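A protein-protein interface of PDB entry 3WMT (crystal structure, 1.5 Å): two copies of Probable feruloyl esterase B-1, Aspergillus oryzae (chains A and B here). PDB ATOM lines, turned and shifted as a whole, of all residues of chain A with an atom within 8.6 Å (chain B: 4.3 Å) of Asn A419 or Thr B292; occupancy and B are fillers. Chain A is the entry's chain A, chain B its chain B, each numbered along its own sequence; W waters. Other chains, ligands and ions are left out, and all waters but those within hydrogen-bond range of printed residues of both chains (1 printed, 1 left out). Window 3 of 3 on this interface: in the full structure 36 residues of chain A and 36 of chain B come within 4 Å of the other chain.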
ATOM      1  N   GLY A 379      13.373  21.281 -21.139  1.00  0.00           N
ATOM      2  CA  GLY A 379      14.151  20.898 -22.328  1.00  0.00           C
ATOM      3  C   GLY A 379      13.473  21.339 -23.596  1.00  0.00           C
ATOM      4  O   GLY A 379      14.066  21.148 -24.643  1.00  0.00           O
ATOM      5  N   ASP A 380      12.241  21.840 -23.556  1.00  0.00           N
ATOM      6  CA  ASP A 380      11.559  22.323 -24.765  1.00  0.00           C
ATOM      7  C   ASP A 380      11.777  23.758 -24.991  1.00  0.00           C
ATOM      8  O   ASP A 380      11.172  24.597 -24.330  1.00  0.00           O
ATOM      9  CB  ASP A 380      10.045  22.051 -24.608  1.00  0.00           C
ATOM     10  CG  ASP A 380       9.282  22.459 -25.777  1.00  0.00           C
ATOM     11  OD1 ASP A 380       9.794  22.876 -26.811  1.00  0.00           O
ATOM     12  OD2 ASP A 380       8.019  22.180 -25.744  1.00  0.00           O
ATOM     13  N   SER A 382      11.274  25.270 -27.933  1.00  0.00           N
ATOM     14  CA  SER A 382      10.602  25.674 -29.186  1.00  0.00           C
ATOM     15  C   SER A 382      10.169  27.139 -29.213  1.00  0.00           C
ATOM     16  O   SER A 382      10.395  27.751 -30.245  1.00  0.00           O
ATOM     17  CB  SER A 382       9.392  24.763 -29.436  1.00  0.00           C
ATOM     18  OG  SER A 382       9.785  23.482 -29.699  1.00  0.00           O
ATOM     19  N   LYS A 412      21.819  16.985 -23.692  1.00  0.00           N
ATOM     20  CA  LYS A 412      21.171  15.764 -24.122  1.00  0.00           C
ATOM     21  C   LYS A 412      19.685  15.761 -23.848  1.00  0.00           C
ATOM     22  O   LYS A 412      18.872  15.338 -24.712  1.00  0.00           O
ATOM     23  CB  LYS A 412      21.799  14.529 -23.441  1.00  0.00           C
ATOM     24  CG  LYS A 412      23.232  14.229 -23.839  1.00  0.00           C
ATOM     25  CD  LYS A 412      23.664  12.947 -23.153  1.00  0.00           C
ATOM     26  CE  LYS A 412      25.061  12.587 -23.416  1.00  0.00           C
ATOM     27  NZ  LYS A 412      25.413  11.191 -22.897  1.00  0.00           N
ATOM     28  N   HIS A 413      19.288  16.367 -22.744  1.00  0.00           N
ATOM     29  CA  HIS A 413      17.893  16.536 -22.402  1.00  0.00           C
ATOM     30  C   HIS A 413      17.144  17.406 -23.407  1.00  0.00           C
ATOM     31  O   HIS A 413      16.018  17.054 -23.838  1.00  0.00           O
ATOM     32  CB  HIS A 413      17.778  17.095 -20.970  1.00  0.00           C
ATOM     33  CG  HIS A 413      16.452  17.512 -20.529  1.00  0.00           C
ATOM     34  ND1 HIS A 413      15.372  16.612 -20.441  1.00  0.00           N
ATOM     35  CD2 HIS A 413      16.051  18.661 -19.951  1.00  0.00           C
ATOM     36  CE1 HIS A 413      14.344  17.278 -19.964  1.00  0.00           C
ATOM     37  NE2 HIS A 413      14.726  18.481 -19.601  1.00  0.00           N
ATOM     38  N   VAL A 414      17.755  18.480 -23.842  1.00  0.00           N
ATOM     39  CA  VAL A 414      17.118  19.336 -24.867  1.00  0.00           C
ATOM     40  C   VAL A 414      16.956  18.552 -26.156  1.00  0.00           C
ATOM     41  O   VAL A 414      15.885  18.542 -26.779  1.00  0.00           O
ATOM     42  CB  VAL A 414      17.934  20.644 -25.086  1.00  0.00           C
ATOM     43  CG1 VAL A 414      17.431  21.390 -26.326  1.00  0.00           C
ATOM     44  CG2 VAL A 414      17.944  21.481 -23.881  1.00  0.00           C
ATOM     45  N   ALA A 415      18.019  17.923 -26.648  1.00  0.00           N
ATOM     46  CA  ALA A 415      17.959  17.160 -27.899  1.00  0.00           C
ATOM     47  C   ALA A 415      16.862  16.145 -27.867  1.00  0.00           C
ATOM     48  O   ALA A 415      16.057  16.033 -28.790  1.00  0.00           O
ATOM     49  CB  ALA A 415      19.318  16.505 -28.218  1.00  0.00           C
ATOM     50  N   ASP A 416      16.864  15.364 -26.817  1.00  0.00           N
ATOM     51  CA  ASP A 416      15.883  14.256 -26.759  1.00  0.00           C
ATOM     52  C   ASP A 416      14.478  14.723 -26.434  1.00  0.00           C
ATOM     53  O   ASP A 416      13.500  14.021 -26.889  1.00  0.00           O
ATOM     54  CB  ASP A 416      16.387  13.246 -25.692  1.00  0.00           C
ATOM     55  CG  ASP A 416      17.721  12.636 -26.059  1.00  0.00           C
ATOM     56  OD1 ASP A 416      17.968  12.470 -27.248  1.00  0.00           O
ATOM     57  OD2 ASP A 416      18.512  12.321 -25.096  1.00  0.00           O
ATOM     58  N   THR A 417      14.311  15.789 -25.700  1.00  0.00           N
ATOM     59  CA  THR A 417      12.966  16.384 -25.460  1.00  0.00           C
ATOM     60  C   THR A 417      12.428  17.032 -26.750  1.00  0.00           C
ATOM     61  O   THR A 417      11.235  16.808 -27.075  1.00  0.00           O
ATOM     62  CB  THR A 417      13.012  17.349 -24.335  1.00  0.00           C
ATOM     63  OG1 THR A 417      13.490  16.764 -23.134  1.00  0.00           O
ATOM     64  CG2 THR A 417      11.671  18.059 -24.092  1.00  0.00           C
ATOM     65  N   MET A 418      13.218  17.788 -27.470  1.00  0.00           N
ATOM     66  CA  MET A 418      12.759  18.384 -28.700  1.00  0.00           C
ATOM     67  C   MET A 418      12.753  17.466 -29.899  1.00  0.00           C
ATOM     68  O   MET A 418      12.230  17.851 -30.971  1.00  0.00           O
ATOM     69  CB  MET A 418      13.616  19.634 -28.975  1.00  0.00           C
ATOM     70  CG  MET A 418      13.505  20.690 -27.915  1.00  0.00           C
ATOM     71  SD  MET A 418      14.358  22.229 -28.322  1.00  0.00           S
ATOM     72  CE  MET A 418      13.215  22.909 -29.558  1.00  0.00           C
ATOM     73  N   ASN A 419      13.324  16.292 -29.770  1.00  0.00           N
ATOM     74  CA  ASN A 419      13.561  15.457 -30.889  1.00  0.00           C
ATOM     75  C   ASN A 419      14.287  16.178 -32.021  1.00  0.00           C
ATOM     76  O   ASN A 419      13.990  15.983 -33.210  1.00  0.00           O
ATOM     77  CB  ASN A 419      12.254  14.812 -31.431  1.00  0.00           C
ATOM     78  CG  ASN A 419      12.379  13.382 -31.342  1.00  0.00           C
ATOM     79  OD1 ASN A 419      13.269  12.798 -32.006  1.00  0.00           O
ATOM     80  ND2 ASN A 419      11.876  12.864 -30.234  1.00  0.00           N
ATOM     81  N   LEU A 420      15.328  16.899 -31.671  1.00  0.00           N
ATOM     82  CA  LEU A 420      16.193  17.606 -32.658  1.00  0.00           C
ATOM     83  C   LEU A 420      17.583  17.051 -32.530  1.00  0.00           C
ATOM     84  O   LEU A 420      18.151  17.021 -31.407  1.00  0.00           O
ATOM     85  CB  LEU A 420      16.167  19.081 -32.394  1.00  0.00           C
ATOM     86  CG  LEU A 420      14.859  19.788 -32.646  1.00  0.00           C
ATOM     87  CD1 LEU A 420      15.013  21.260 -32.359  1.00  0.00           C
ATOM     88  CD2 LEU A 420      14.289  19.563 -34.060  1.00  0.00           C
ATOM     89  N   SER A 421      18.218  16.700 -33.680  1.00  0.00           N
ATOM     90  CA  SER A 421      19.571  16.303 -33.676  1.00  0.00           C
ATOM     91  C   SER A 421      20.546  17.465 -33.355  1.00  0.00           C
ATOM     92  O   SER A 421      20.153  18.617 -33.412  1.00  0.00           O
ATOM     93  CB  SER A 421      19.924  15.767 -35.038  1.00  0.00           C
ATOM     94  OG  SER A 421      19.944  16.841 -35.971  1.00  0.00           O
ATOM     95  N   PRO A 422      21.802  17.144 -32.964  1.00  0.00           N
ATOM     96  CA  PRO A 422      22.747  18.225 -32.681  1.00  0.00           C
ATOM     97  C   PRO A 422      22.835  19.168 -33.846  1.00  0.00           C
ATOM     98  O   PRO A 422      22.909  20.374 -33.622  1.00  0.00           O
ATOM     99  CB  PRO A 422      24.026  17.435 -32.363  1.00  0.00           C
ATOM    100  CG  PRO A 422      23.468  16.141 -31.758  1.00  0.00           C
ATOM    101  CD  PRO A 422      22.350  15.829 -32.667  1.00  0.00           C
ATOM    102  N   GLU A 424      20.610  19.982 -36.022  1.00  0.00           N
ATOM    103  CA  GLU A 424      19.398  20.783 -35.969  1.00  0.00           C
ATOM    104  C   GLU A 424      19.458  21.793 -34.864  1.00  0.00           C
ATOM    105  O   GLU A 424      19.108  22.961 -35.081  1.00  0.00           O
ATOM    106  CB  GLU A 424      18.097  19.910 -35.863  1.00  0.00           C
ATOM    107  CG  GLU A 424      17.828  19.126 -37.111  1.00  0.00           C
ATOM    108  CD  GLU A 424      16.748  18.124 -36.971  1.00  0.00           C
ATOM    109  OE1 GLU A 424      16.499  17.546 -35.908  1.00  0.00           O
ATOM    110  OE2 GLU A 424      16.088  17.803 -38.022  1.00  0.00           O
ATOM    111  N   LEU A 425      19.827  21.389 -33.648  1.00  0.00           N
ATOM    112  CA  LEU A 425      19.944  22.349 -32.549  1.00  0.00           C
ATOM    113  C   LEU A 425      20.908  23.451 -32.900  1.00  0.00           C
ATOM    114  O   LEU A 425      20.726  24.564 -32.431  1.00  0.00           O
ATOM    115  CB  LEU A 425      20.438  21.601 -31.253  1.00  0.00           C
ATOM    116  CG  LEU A 425      19.409  20.671 -30.574  1.00  0.00           C
ATOM    117  CD1 LEU A 425      20.111  20.092 -29.419  1.00  0.00           C
ATOM    118  CD2 LEU A 425      18.209  21.467 -30.145  1.00  0.00           C
ATOM    119  N   LEU B 278      20.356  11.027 -33.431  1.00  0.00           N
ATOM    120  CA  LEU B 278      19.013  11.580 -33.682  1.00  0.00           C
ATOM    121  C   LEU B 278      18.883  11.926 -35.219  1.00  0.00           C
ATOM    122  O   LEU B 278      19.759  12.411 -35.852  1.00  0.00           O
ATOM    123  CB  LEU B 278      18.847  12.816 -32.817  1.00  0.00           C
ATOM    124  CG  LEU B 278      18.577  12.536 -31.358  1.00  0.00           C
ATOM    125  CD1 LEU B 278      18.816  13.798 -30.516  1.00  0.00           C
ATOM    126  CD2 LEU B 278      17.173  12.034 -31.095  1.00  0.00           C
ATOM    127  N   SER B 285      13.342   7.487 -38.648  1.00  0.00           N
ATOM    128  CA  SER B 285      13.874   6.395 -37.789  1.00  0.00           C
ATOM    129  C   SER B 285      13.455   5.012 -38.361  1.00  0.00           C
ATOM    130  O   SER B 285      14.101   4.008 -38.111  1.00  0.00           O
ATOM    131  CB  SER B 285      13.430   6.488 -36.381  1.00  0.00           C
ATOM    132  OG  SER B 285      12.015   6.398 -36.245  1.00  0.00           O
ATOM    133  N   LEU B 291      17.587   7.504 -34.706  1.00  0.00           N
ATOM    134  CA  LEU B 291      16.704   7.261 -33.635  1.00  0.00           C
ATOM    135  C   LEU B 291      15.882   8.489 -33.270  1.00  0.00           C
ATOM    136  O   LEU B 291      16.355   9.619 -33.471  1.00  0.00           O
ATOM    137  CB  LEU B 291      17.518   6.878 -32.378  1.00  0.00           C
ATOM    138  CG  LEU B 291      18.021   5.414 -32.302  1.00  0.00           C
ATOM    139  CD1 LEU B 291      18.917   5.016 -33.327  1.00  0.00           C
ATOM    140  CD2 LEU B 291      18.678   5.126 -30.968  1.00  0.00           C
ATOM    141  N   THR B 292      14.706   8.284 -32.707  1.00  0.00           N
ATOM    142  CA  THR B 292      13.950   9.284 -32.081  1.00  0.00           C
ATOM    143  C   THR B 292      14.484   9.664 -30.715  1.00  0.00           C
ATOM    144  O   THR B 292      15.245   8.877 -30.055  1.00  0.00           O
ATOM    145  CB  THR B 292      12.484   8.898 -31.857  1.00  0.00           C
ATOM    146  OG1 THR B 292      12.366   7.856 -30.873  1.00  0.00           O
ATOM    147  CG2 THR B 292      11.764   8.440 -33.169  1.00  0.00           C
ATOM    148  N   GLY B 293      14.051  10.756 -30.117  1.00  0.00           N
ATOM    149  CA  GLY B 293      14.431  11.096 -28.739  1.00  0.00           C
ATOM    150  C   GLY B 293      14.084  10.063 -27.752  1.00  0.00           C
ATOM    151  O   GLY B 293      14.883   9.745 -26.823  1.00  0.00           O
ATOM    152  N   ALA B 294      12.908   9.482 -27.898  1.00  0.00           N
ATOM    153  CA  ALA B 294      12.525   8.407 -26.957  1.00  0.00           C
ATOM    154  C   ALA B 294      13.396   7.220 -27.050  1.00  0.00           C
ATOM    155  O   ALA B 294      13.764   6.615 -26.023  1.00  0.00           O
ATOM    156  CB  ALA B 294      11.087   7.969 -27.221  1.00  0.00           C
ATOM    157  N   GLN B 295      13.798   6.876 -28.269  1.00  0.00           N
ATOM    158  CA  GLN B 295      14.679   5.738 -28.521  1.00  0.00           C
ATOM    159  C   GLN B 295      16.080   6.035 -27.945  1.00  0.00           C
ATOM    160  O   GLN B 295      16.730   5.136 -27.357  1.00  0.00           O
ATOM    161  CB  GLN B 295      14.695   5.406 -29.983  1.00  0.00           C
ATOM    162  CG  GLN B 295      13.348   4.782 -30.476  1.00  0.00           C
ATOM    163  CD  GLN B 295      13.171   4.924 -31.935  1.00  0.00           C
ATOM    164  OE1 GLN B 295      13.913   5.441 -32.715  1.00  0.00           O
ATOM    165  NE2 GLN B 295      11.959   4.448 -32.286  1.00  0.00           N
ATOM    166  N   VAL B 296      16.590   7.225 -28.164  1.00  0.00           N
ATOM    167  CA  VAL B 296      17.834   7.607 -27.547  1.00  0.00           C
ATOM    168  C   VAL B 296      17.800   7.478 -26.045  1.00  0.00           C
ATOM    169  O   VAL B 296      18.766   6.961 -25.431  1.00  0.00           O
ATOM    170  CB  VAL B 296      18.280   9.022 -28.004  1.00  0.00           C
ATOM    171  CG1 VAL B 296      19.523   9.443 -27.190  1.00  0.00           C
ATOM    172  CG2 VAL B 296      18.567   9.045 -29.460  1.00  0.00           C
HETATM  173  O   HOH W   1      14.562  11.784 -34.344  1.00  0.00           O
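Water W1 lies within hydrogen-bond range of OD1 of Asn A419 (2.9 Å) and O of Leu B291 (2.9 Å).
The backbone NH (N) of Gly B293 is in hydrogen-bond range of the side-chain amide oxygen (OD1) of Asn A419, at 2.9 Å.
The backbone NH (N) of Leu A420 sits at hydrogen-bond distance from the backbone carbonyl oxygen (O) of Ala A415, 3.1 Å away.
N of Ser A421 sits at hydrogen-bond distance from OE1 of Glu A424 (2.9 Å).
The side-chain hydroxyl of Thr B292 sits close to the backbone NH of Ala B294, 3.4 Å away.
OE1 of Gln B295 lies within hydrogen-bond range of N of Thr B292.
Of chain B, only Thr B292 and Gly B293 come within 4 Å of Asn A419.
Thr B292 touches just one residue of chain A: Asn A419.
Gly B293 touches two residues of chain A.
Of the printed residues of chain B, Leu A420 touches Leu B278 (3.4 Å).
Of the printed residues of chain A, Val B296 touches Asp A416 (3.4 Å).
The nearest residue of chain A that does not touch Thr B292 is Asp A416 (5.3 Å).
The nearest printed residue of chain B that does not touch Asp A416 is Ala B294 (4.7 Å).
Of the 16 printed residues of chain A, 5 touch a printed residue of chain B.
Printed residues of chain A that touch a printed residue of chain B: Ala A415, Asp A416, Asn A419, Leu A420 and Ser A421.
Along chain A the printed residues that touch a printed residue of chain B span positions 415 to 421.
Of the 8 printed residues of chain B, 4 touch a printed residue of chain A.
Hydrophobic or aromatic side chains of chain B within 4 Å of the printed part of chain A: Leu B278 and Val B296.
Among the printed residues, 8 pairs touch across the chains.
Ala A415 touches Leu B278.
Leu B278 touches Asp A416 (CD1 to OD1, 3.6 Å).
Gly B293 touches Asp A416 (CA to O, 3.6 Å).
Asp A416 touches Val B296.
Thr B292 touches Asn A419.
Leu A420 touches Leu B278.
Leu B278 touches Ser A421.
No position is printed for both chains.
Of the 8 pairs that touch across the chains among the printed residues, none has its exchanged pair printed and touching as well.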
